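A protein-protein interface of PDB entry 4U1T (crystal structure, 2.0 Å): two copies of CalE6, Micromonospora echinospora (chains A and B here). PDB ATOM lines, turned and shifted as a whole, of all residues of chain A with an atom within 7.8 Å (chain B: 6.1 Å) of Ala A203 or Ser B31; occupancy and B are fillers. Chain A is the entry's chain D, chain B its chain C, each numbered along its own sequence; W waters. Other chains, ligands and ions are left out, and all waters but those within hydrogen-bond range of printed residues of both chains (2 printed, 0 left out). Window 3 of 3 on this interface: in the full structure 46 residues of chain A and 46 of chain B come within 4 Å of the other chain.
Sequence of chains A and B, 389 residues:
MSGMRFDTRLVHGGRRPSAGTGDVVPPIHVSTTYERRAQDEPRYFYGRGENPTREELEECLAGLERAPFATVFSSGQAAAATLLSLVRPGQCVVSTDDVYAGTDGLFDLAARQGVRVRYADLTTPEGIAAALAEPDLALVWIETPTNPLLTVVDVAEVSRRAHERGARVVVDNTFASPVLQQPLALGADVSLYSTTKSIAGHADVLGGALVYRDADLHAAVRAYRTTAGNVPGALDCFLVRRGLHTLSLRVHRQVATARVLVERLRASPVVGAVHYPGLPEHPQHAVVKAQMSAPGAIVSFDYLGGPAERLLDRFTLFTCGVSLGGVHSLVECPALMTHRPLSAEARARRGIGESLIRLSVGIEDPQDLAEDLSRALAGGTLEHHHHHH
The backbone carbonyl oxygen (O) of Val A322 sits at hydrogen-bond distance from the side-chain hydroxyl (OG1) of Thr B33.
N of Thr B32 is in hydrogen-bond range of O of Ala A203 (2.9 Å).
The backbone carbonyl oxygen (O) of Asp A204 sits close to the backbone carbonyl oxygen (O) of Val B30, at 3.3 Å.
OG of Ser B31 is in hydrogen-bond range of O of Thr B33 (2.7 Å).
OG1 of Thr A196 sits at hydrogen-bond distance from OP3 of LLP A197 (2.7 Å).
The backbone NH (N) of Gly B47 lies within hydrogen-bond range of the backbone carbonyl oxygen (O) of Thr B32 (2.8 Å).
Among the printed residues, merely in contact across the chains: Thr A196 with Thr B32, Ala A203 with Val B30, Ala A203 with Ser B31, Asp A204 with Thr B32 and Val A205 with Thr B32.
Ala A203 touches just these residues of chain B: Val B30 (3.9 Å), Ser B31 (3.4 Å) and Thr B32 (2.9 Å).
Ser B31 touches just one residue of chain A: Ala A203 (3.4 Å).
Of the printed residues of chain B, Val A322 touches Thr B33 (2.8 Å).
Printed residues of chain A within 4 Å of Val B30: Ala A203 (3.9 Å) and Asp A204 (3.2 Å).
Of the printed residues of chain A, Thr B33 touches Val A322.
Of the printed residues of chain B, Thr A196 touches Thr B32.
Val A327 touches none of the printed residues of chain B.
Gly A325 touches none of the printed residues of chain B.
The nearest residue of chain A that does not touch Ser B31 is Asp A204 (4.5 Å).
Of the 19 printed residues of chain A, 5 touch a printed residue of chain B.
Hydrophobic or aromatic side chains of chain A within 4 Å of the printed part of chain B: Ala A203.
Of the 10 printed residues of chain B, 4 touch a printed residue of chain A.
Hydrophobic or aromatic side chains of chain B within 4 Å of the printed part of chain A: Val B30.
Among the printed residues, no Asp or Glu carboxylate lies within 4 Å of a Lys or Arg side-chain nitrogen of the other chain.
No position is printed for both chains.
Water W2 lies within hydrogen-bond range of the side-chain hydroxyl (OG) of Ser A323 (2.7 Å), the side-chain hydroxyl (OG1) of Thr B32 (2.7 Å) and the backbone carbonyl oxygen (O) of Thr A196 (3.2 Å).
Water W1 bridges the backbone carbonyl oxygen of Tyr B34 (2.8 Å) and the backbone NH of Val A322 (3.0 Å).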
ATOM      1  N   THR A 195      12.188  -0.199  -2.638  1.00  0.00           N
ATOM      2  CA  THR A 195      10.894  -0.570  -3.205  1.00  0.00           C
ATOM      3  C   THR A 195      10.744  -2.086  -3.244  1.00  0.00           C
ATOM      4  O   THR A 195       9.655  -2.598  -3.472  1.00  0.00           O
ATOM      5  CB  THR A 195      10.674   0.031  -4.607  1.00  0.00           C
ATOM      6  OG1 THR A 195      11.708  -0.395  -5.500  1.00  0.00           O
ATOM      7  CG2 THR A 195      10.675   1.571  -4.521  1.00  0.00           C
ATOM      8  N   THR A 196      11.850  -2.786  -3.007  1.00  0.00           N
ATOM      9  CA  THR A 196      11.871  -4.234  -2.814  1.00  0.00           C
ATOM     10  C   THR A 196      10.837  -4.706  -1.789  1.00  0.00           C
ATOM     11  O   THR A 196      10.323  -5.816  -1.879  1.00  0.00           O
ATOM     12  CB  THR A 196      13.257  -4.694  -2.342  1.00  0.00           C
ATOM     13  OG1 THR A 196      14.274  -4.159  -3.208  1.00  0.00           O
ATOM     14  CG2 THR A 196      13.349  -6.225  -2.282  1.00  0.00           C
ATOM     15  N1  LLP A 197      16.431   0.365   4.144  1.00  0.00           N
ATOM     16  C2  LLP A 197      15.569  -0.438   4.775  1.00  0.00           C
ATOM     17  C2' LLP A 197      14.769   0.067   6.016  1.00  0.00           C
ATOM     18  C3  LLP A 197      15.369  -1.767   4.307  1.00  0.00           C
ATOM     19  O3  LLP A 197      14.456  -2.587   4.984  1.00  0.00           O
ATOM     20  C4  LLP A 197      16.059  -2.248   3.204  1.00  0.00           C
ATOM     21  C4' LLP A 197      15.762  -3.778   2.746  1.00  0.00           C
ATOM     22  C5  LLP A 197      16.963  -1.424   2.565  1.00  0.00           C
ATOM     23  C6  LLP A 197      17.152  -0.106   3.032  1.00  0.00           C
ATOM     24  C5' LLP A 197      17.806  -1.863   1.311  1.00  0.00           C
ATOM     25  OP4 LLP A 197      16.953  -2.229   0.241  1.00  0.00           O
ATOM     26  P   LLP A 197      17.392  -3.227  -0.865  1.00  0.00           P
ATOM     27  OP1 LLP A 197      17.388  -4.636  -0.328  1.00  0.00           O
ATOM     28  OP2 LLP A 197      18.747  -2.849  -1.324  1.00  0.00           O
ATOM     29  OP3 LLP A 197      16.419  -3.144  -2.001  1.00  0.00           O
ATOM     30  N   LLP A 197      10.555  -3.860  -0.805  1.00  0.00           N
ATOM     31  CA  LLP A 197       9.697  -4.242   0.331  1.00  0.00           C
ATOM     32  CB  LLP A 197      10.188  -3.525   1.582  1.00  0.00           C
ATOM     33  CG  LLP A 197      11.724  -3.587   1.698  1.00  0.00           C
ATOM     34  CD  LLP A 197      12.252  -5.000   2.013  1.00  0.00           C
ATOM     35  CE  LLP A 197      13.812  -5.041   2.027  1.00  0.00           C
ATOM     36  NZ  LLP A 197      14.404  -4.176   3.064  1.00  0.00           N
ATOM     37  C   LLP A 197       8.237  -4.009  -0.008  1.00  0.00           C
ATOM     38  O   LLP A 197       7.751  -4.618  -0.949  1.00  0.00           O
ATOM     39  N   SER A 198       7.526  -3.141   0.719  1.00  0.00           N
ATOM     40  CA  SER A 198       6.069  -3.051   0.531  1.00  0.00           C
ATOM     41  C   SER A 198       5.640  -2.365  -0.767  1.00  0.00           C
ATOM     42  O   SER A 198       4.571  -2.676  -1.291  1.00  0.00           O
ATOM     43  CB  SER A 198       5.405  -2.354   1.733  1.00  0.00           C
ATOM     44  OG  SER A 198       5.910  -1.045   1.954  1.00  0.00           O
ATOM     45  N   ALA A 200       6.769  -2.541  -4.056  1.00  0.00           N
ATOM     46  CA  ALA A 200       6.508  -3.593  -5.052  1.00  0.00           C
ATOM     47  C   ALA A 200       5.612  -4.685  -4.432  1.00  0.00           C
ATOM     48  O   ALA A 200       4.665  -5.172  -5.068  1.00  0.00           O
ATOM     49  CB  ALA A 200       7.825  -4.186  -5.578  1.00  0.00           C
ATOM     50  N   GLY A 201       5.925  -5.074  -3.194  1.00  0.00           N
ATOM     51  CA  GLY A 201       4.989  -5.809  -2.356  1.00  0.00           C
ATOM     52  C   GLY A 201       4.816  -7.316  -2.546  1.00  0.00           C
ATOM     53  O   GLY A 201       4.107  -7.949  -1.766  1.00  0.00           O
ATOM     54  N   HIS A 202       5.453  -7.900  -3.557  1.00  0.00           N
ATOM     55  CA  HIS A 202       5.211  -9.312  -3.879  1.00  0.00           C
ATOM     56  C   HIS A 202       6.485 -10.168  -3.838  1.00  0.00           C
ATOM     57  O   HIS A 202       6.510 -11.290  -4.362  1.00  0.00           O
ATOM     58  CB  HIS A 202       4.520  -9.404  -5.256  1.00  0.00           C
ATOM     59  CG  HIS A 202       3.162  -8.759  -5.284  1.00  0.00           C
ATOM     60  ND1 HIS A 202       2.987  -7.389  -5.214  1.00  0.00           N
ATOM     61  CD2 HIS A 202       1.916  -9.292  -5.355  1.00  0.00           C
ATOM     62  CE1 HIS A 202       1.693  -7.107  -5.259  1.00  0.00           C
ATOM     63  NE2 HIS A 202       1.021  -8.244  -5.354  1.00  0.00           N
ATOM     64  N   ALA A 203       7.542  -9.618  -3.239  1.00  0.00           N
ATOM     65  CA  ALA A 203       8.809 -10.332  -3.014  1.00  0.00           C
ATOM     66  C   ALA A 203       9.429 -10.924  -4.285  1.00  0.00           C
ATOM     67  O   ALA A 203      10.063 -11.982  -4.232  1.00  0.00           O
ATOM     68  CB  ALA A 203       8.603 -11.453  -1.950  1.00  0.00           C
ATOM     69  N   ASP A 204       9.286 -10.237  -5.415  1.00  0.00           N
ATOM     70  CA  ASP A 204       9.764 -10.789  -6.684  1.00  0.00           C
ATOM     71  C   ASP A 204      10.538  -9.779  -7.546  1.00  0.00           C
ATOM     72  O   ASP A 204      10.713  -9.976  -8.755  1.00  0.00           O
ATOM     73  CB  ASP A 204       8.587 -11.370  -7.484  1.00  0.00           C
ATOM     74  CG  ASP A 204       7.470 -10.338  -7.767  1.00  0.00           C
ATOM     75  OD1 ASP A 204       7.685  -9.114  -7.589  1.00  0.00           O
ATOM     76  OD2 ASP A 204       6.360 -10.764  -8.178  1.00  0.00           O
ATOM     77  N   VAL A 205      11.024  -8.705  -6.930  1.00  0.00           N
ATOM     78  CA  VAL A 205      11.825  -7.735  -7.680  1.00  0.00           C
ATOM     79  C   VAL A 205      12.595  -6.855  -6.681  1.00  0.00           C
ATOM     80  O   VAL A 205      12.097  -6.567  -5.589  1.00  0.00           O
ATOM     81  CB  VAL A 205      10.945  -6.877  -8.636  1.00  0.00           C
ATOM     82  CG1 VAL A 205       9.902  -6.048  -7.861  1.00  0.00           C
ATOM     83  CG2 VAL A 205      11.810  -5.986  -9.540  1.00  0.00           C
ATOM     84  N   LEU A 206      13.825  -6.487  -7.044  1.00  0.00           N
ATOM     85  CA  LEU A 206      14.643  -5.553  -6.259  1.00  0.00           C
ATOM     86  C   LEU A 206      14.510  -4.143  -6.811  1.00  0.00           C
ATOM     87  O   LEU A 206      14.470  -3.960  -8.020  1.00  0.00           O
ATOM     88  CB  LEU A 206      16.120  -5.940  -6.287  1.00  0.00           C
ATOM     89  CG  LEU A 206      16.542  -7.291  -5.716  1.00  0.00           C
ATOM     90  CD1 LEU A 206      18.034  -7.504  -5.972  1.00  0.00           C
ATOM     91  CD2 LEU A 206      16.242  -7.338  -4.230  1.00  0.00           C
ATOM     92  N   VAL A 322      14.499 -13.310   5.699  1.00  0.00           N
ATOM     93  CA  VAL A 322      14.679 -11.876   5.843  1.00  0.00           C
ATOM     94  C   VAL A 322      13.815 -11.181   4.807  1.00  0.00           C
ATOM     95  O   VAL A 322      13.114 -11.849   4.042  1.00  0.00           O
ATOM     96  CB  VAL A 322      16.161 -11.458   5.685  1.00  0.00           C
ATOM     97  CG1 VAL A 322      17.016 -12.182   6.710  1.00  0.00           C
ATOM     98  CG2 VAL A 322      16.660 -11.759   4.272  1.00  0.00           C
ATOM     99  N   SER A 323      13.887  -9.851   4.808  1.00  0.00           N
ATOM    100  CA  SER A 323      13.047  -8.936   4.032  1.00  0.00           C
ATOM    101  C   SER A 323      11.722  -8.705   4.736  1.00  0.00           C
ATOM    102  O   SER A 323      11.444  -9.278   5.798  1.00  0.00           O
ATOM    103  CB  SER A 323      12.805  -9.427   2.594  1.00  0.00           C
ATOM    104  OG  SER A 323      12.408  -8.348   1.754  1.00  0.00           O
ATOM    105  N   LEU A 324      10.908  -7.834   4.150  1.00  0.00           N
ATOM    106  CA  LEU A 324       9.677  -7.417   4.795  1.00  0.00           C
ATOM    107  C   LEU A 324       8.765  -6.717   3.798  1.00  0.00           C
ATOM    108  O   LEU A 324       9.163  -6.472   2.656  1.00  0.00           O
ATOM    109  CB  LEU A 324       9.989  -6.500   5.970  1.00  0.00           C
ATOM    110  CG  LEU A 324      10.834  -5.281   5.621  1.00  0.00           C
ATOM    111  CD1 LEU A 324      10.005  -4.001   5.682  1.00  0.00           C
ATOM    112  CD2 LEU A 324      12.047  -5.212   6.540  1.00  0.00           C
ATOM    113  N   GLY A 325       7.545  -6.427   4.233  1.00  0.00           N
ATOM    114  CA  GLY A 325       6.623  -5.617   3.457  1.00  0.00           C
ATOM    115  C   GLY A 325       5.787  -6.409   2.463  1.00  0.00           C
ATOM    116  O   GLY A 325       4.831  -5.884   1.912  1.00  0.00           O
ATOM    117  N   GLY A 326       6.140  -7.672   2.235  1.00  0.00           N
ATOM    118  CA  GLY A 326       5.492  -8.459   1.191  1.00  0.00           C
ATOM    119  C   GLY A 326       4.150  -9.101   1.531  1.00  0.00           C
ATOM    120  O   GLY A 326       3.705  -9.067   2.679  1.00  0.00           O
ATOM    121  N   VAL A 327       3.505  -9.703   0.529  1.00  0.00           N
ATOM    122  CA  VAL A 327       2.209 -10.362   0.754  1.00  0.00           C
ATOM    123  C   VAL A 327       2.343 -11.582   1.671  1.00  0.00           C
ATOM    124  O   VAL A 327       1.389 -11.949   2.357  1.00  0.00           O
ATOM    125  CB  VAL A 327       1.552 -10.782  -0.590  1.00  0.00           C
ATOM    126  CG1 VAL A 327       1.126  -9.555  -1.399  1.00  0.00           C
ATOM    127  CG2 VAL A 327       2.485 -11.676  -1.417  1.00  0.00           C
ATOM    128  N   HIS A 328       3.529 -12.201   1.687  1.00  0.00           N
ATOM    129  CA  HIS A 328       3.782 -13.359   2.553  1.00  0.00           C
ATOM    130  C   HIS A 328       4.305 -12.887   3.899  1.00  0.00           C
ATOM    131  O   HIS A 328       5.281 -12.128   3.939  1.00  0.00           O
ATOM    132  CB  HIS A 328       4.821 -14.333   1.953  1.00  0.00           C
ATOM    133  CG  HIS A 328       4.843 -14.389   0.458  1.00  0.00           C
ATOM    134  ND1 HIS A 328       5.488 -13.444  -0.313  1.00  0.00           N
ATOM    135  CD2 HIS A 328       4.347 -15.309  -0.408  1.00  0.00           C
ATOM    136  CE1 HIS A 328       5.350 -13.751  -1.591  1.00  0.00           C
ATOM    137  NE2 HIS A 328       4.671 -14.885  -1.675  1.00  0.00           N
ATOM    138  N   LEU A 330       6.466 -12.853   7.183  1.00  0.00           N
ATOM    139  CA  LEU A 330       7.835 -13.314   7.441  1.00  0.00           C
ATOM    140  C   LEU A 330       8.196 -13.161   8.918  1.00  0.00           C
ATOM    141  O   LEU A 330       7.703 -12.264   9.598  1.00  0.00           O
ATOM    142  CB  LEU A 330       8.834 -12.531   6.577  1.00  0.00           C
ATOM    143  CG  LEU A 330       8.674 -12.640   5.054  1.00  0.00           C
ATOM    144  CD1 LEU A 330       9.478 -11.567   4.335  1.00  0.00           C
ATOM    145  CD2 LEU A 330       9.165 -14.009   4.597  1.00  0.00           C
ATOM    146  N   ILE B  28      13.446 -19.143 -13.940  1.00  0.00           N
ATOM    147  CA  ILE B  28      13.884 -17.796 -13.582  1.00  0.00           C
ATOM    148  C   ILE B  28      13.590 -17.530 -12.112  1.00  0.00           C
ATOM    149  O   ILE B  28      12.429 -17.505 -11.701  1.00  0.00           O
ATOM    150  CB  ILE B  28      13.187 -16.715 -14.445  1.00  0.00           C
ATOM    151  CG1 ILE B  28      13.315 -17.057 -15.929  1.00  0.00           C
ATOM    152  CG2 ILE B  28      13.775 -15.329 -14.145  1.00  0.00           C
ATOM    153  CD1 ILE B  28      12.520 -16.120 -16.861  1.00  0.00           C
ATOM    154  N   HIS B  29      14.641 -17.336 -11.319  1.00  0.00           N
ATOM    155  CA  HIS B  29      14.474 -17.125  -9.880  1.00  0.00           C
ATOM    156  C   HIS B  29      14.210 -15.667  -9.559  1.00  0.00           C
ATOM    157  O   HIS B  29      15.149 -14.884  -9.456  1.00  0.00           O
ATOM    158  CB  HIS B  29      15.709 -17.620  -9.138  1.00  0.00           C
ATOM    159  CG  HIS B  29      15.859 -19.108  -9.196  1.00  0.00           C
ATOM    160  ND1 HIS B  29      15.407 -19.936  -8.196  1.00  0.00           N
ATOM    161  CD2 HIS B  29      16.364 -19.915 -10.159  1.00  0.00           C
ATOM    162  CE1 HIS B  29      15.639 -21.195  -8.532  1.00  0.00           C
ATOM    163  NE2 HIS B  29      16.225 -21.209  -9.716  1.00  0.00           N
ATOM    164  N   VAL B  30      12.936 -15.304  -9.420  1.00  0.00           N
ATOM    165  CA  VAL B  30      12.577 -13.906  -9.160  1.00  0.00           C
ATOM    166  C   VAL B  30      12.474 -13.584  -7.674  1.00  0.00           C
ATOM    167  O   VAL B  30      12.491 -12.414  -7.303  1.00  0.00           O
ATOM    168  CB  VAL B  30      11.240 -13.522  -9.836  1.00  0.00           C
ATOM    169  CG1 VAL B  30      11.377 -13.532 -11.367  1.00  0.00           C
ATOM    170  CG2 VAL B  30      10.102 -14.456  -9.368  1.00  0.00           C
ATOM    171  N   SER B  31      12.364 -14.606  -6.827  1.00  0.00           N
ATOM    172  CA  SER B  31      12.127 -14.385  -5.390  1.00  0.00           C
ATOM    173  C   SER B  31      13.241 -13.537  -4.761  1.00  0.00           C
ATOM    174  O   SER B  31      14.419 -13.785  -4.997  1.00  0.00           O
ATOM    175  CB  SER B  31      12.007 -15.718  -4.635  1.00  0.00           C
ATOM    176  OG  SER B  31      11.551 -15.533  -3.288  1.00  0.00           O
ATOM    177  N   THR B  32      12.860 -12.543  -3.962  1.00  0.00           N
ATOM    178  CA  THR B  32      13.842 -11.723  -3.243  1.00  0.00           C
ATOM    179  C   THR B  32      14.293 -12.396  -1.962  1.00  0.00           C
ATOM    180  O   THR B  32      15.343 -12.075  -1.412  1.00  0.00           O
ATOM    181  CB  THR B  32      13.261 -10.362  -2.846  1.00  0.00           C
ATOM    182  OG1 THR B  32      12.149 -10.585  -1.978  1.00  0.00           O
ATOM    183  CG2 THR B  32      12.799  -9.595  -4.061  1.00  0.00           C
ATOM    184  N   THR B  33      13.471 -13.298  -1.449  1.00  0.00           N
ATOM    185  CA  THR B  33      13.825 -13.915  -0.185  1.00  0.00           C
ATOM    186  C   THR B  33      13.662 -15.428  -0.214  1.00  0.00           C
ATOM    187  O   THR B  33      13.056 -15.998  -1.140  1.00  0.00           O
ATOM    188  CB  THR B  33      13.044 -13.312   0.991  1.00  0.00           C
ATOM    189  OG1 THR B  33      13.542 -13.878   2.216  1.00  0.00           O
ATOM    190  CG2 THR B  33      11.559 -13.562   0.855  1.00  0.00           C
ATOM    191  N   TYR B  34      14.274 -16.067   0.780  1.00  0.00           N
ATOM    192  CA  TYR B  34      14.411 -17.513   0.836  1.00  0.00           C
ATOM    193  C   TYR B  34      14.067 -18.020   2.212  1.00  0.00           C
ATOM    194  O   TYR B  34      14.419 -17.389   3.214  1.00  0.00           O
ATOM    195  CB  TYR B  34      15.834 -17.920   0.499  1.00  0.00           C
ATOM    196  CG  TYR B  34      16.296 -17.433  -0.838  1.00  0.00           C
ATOM    197  CD1 TYR B  34      16.955 -16.213  -0.957  1.00  0.00           C
ATOM    198  CD2 TYR B  34      16.065 -18.173  -1.987  1.00  0.00           C
ATOM    199  CE1 TYR B  34      17.380 -15.755  -2.173  1.00  0.00           C
ATOM    200  CE2 TYR B  34      16.486 -17.722  -3.208  1.00  0.00           C
ATOM    201  CZ  TYR B  34      17.153 -16.511  -3.297  1.00  0.00           C
ATOM    202  OH  TYR B  34      17.589 -16.042  -4.515  1.00  0.00           O
ATOM    203  N   GLY B  47      18.011 -11.759  -2.052  1.00  0.00           N
ATOM    204  CA  GLY B  47      18.261 -11.624  -3.475  1.00  0.00           C
ATOM    205  C   GLY B  47      19.380 -10.674  -3.864  1.00  0.00           C
ATOM    206  O   GLY B  47      20.041 -10.883  -4.881  1.00  0.00           O
ATOM    207  N   GLU B  50      22.424 -13.054  -3.027  1.00  0.00           N
ATOM    208  CA  GLU B  50      22.478 -14.356  -3.706  1.00  0.00           C
ATOM    209  C   GLU B  50      21.257 -14.552  -4.599  1.00  0.00           C
ATOM    210  O   GLU B  50      20.136 -14.257  -4.189  1.00  0.00           O
ATOM    211  CB  GLU B  50      22.532 -15.516  -2.696  1.00  0.00           C
ATOM    212  CG  GLU B  50      23.576 -15.409  -1.593  1.00  0.00           C
ATOM    213  CD  GLU B  50      23.139 -14.488  -0.472  1.00  0.00           C
ATOM    214  OE1 GLU B  50      23.983 -13.691  -0.015  1.00  0.00           O
ATOM    215  OE2 GLU B  50      21.958 -14.560  -0.044  1.00  0.00           O
ATOM    216  N   ASN B  51      21.468 -15.099  -5.790  1.00  0.00           N
ATOM    217  CA  ASN B  51      20.373 -15.413  -6.704  1.00  0.00           C
ATOM    218  C   ASN B  51      20.845 -16.455  -7.706  1.00  0.00           C
ATOM    219  O   ASN B  51      21.861 -16.256  -8.358  1.00  0.00           O
ATOM    220  CB  ASN B  51      19.890 -14.166  -7.442  1.00  0.00           C
ATOM    221  CG  ASN B  51      18.786 -14.483  -8.456  1.00  0.00           C
ATOM    222  OD1 ASN B  51      19.059 -14.978  -9.545  1.00  0.00           O
ATOM    223  ND2 ASN B  51      17.546 -14.188  -8.102  1.00  0.00           N
HETATM  224  O   HOH W   1      16.078 -15.366   4.145  1.00  0.00           O
HETATM  225  O   HOH W   2      11.030  -8.570  -0.503  1.00  0.00           O
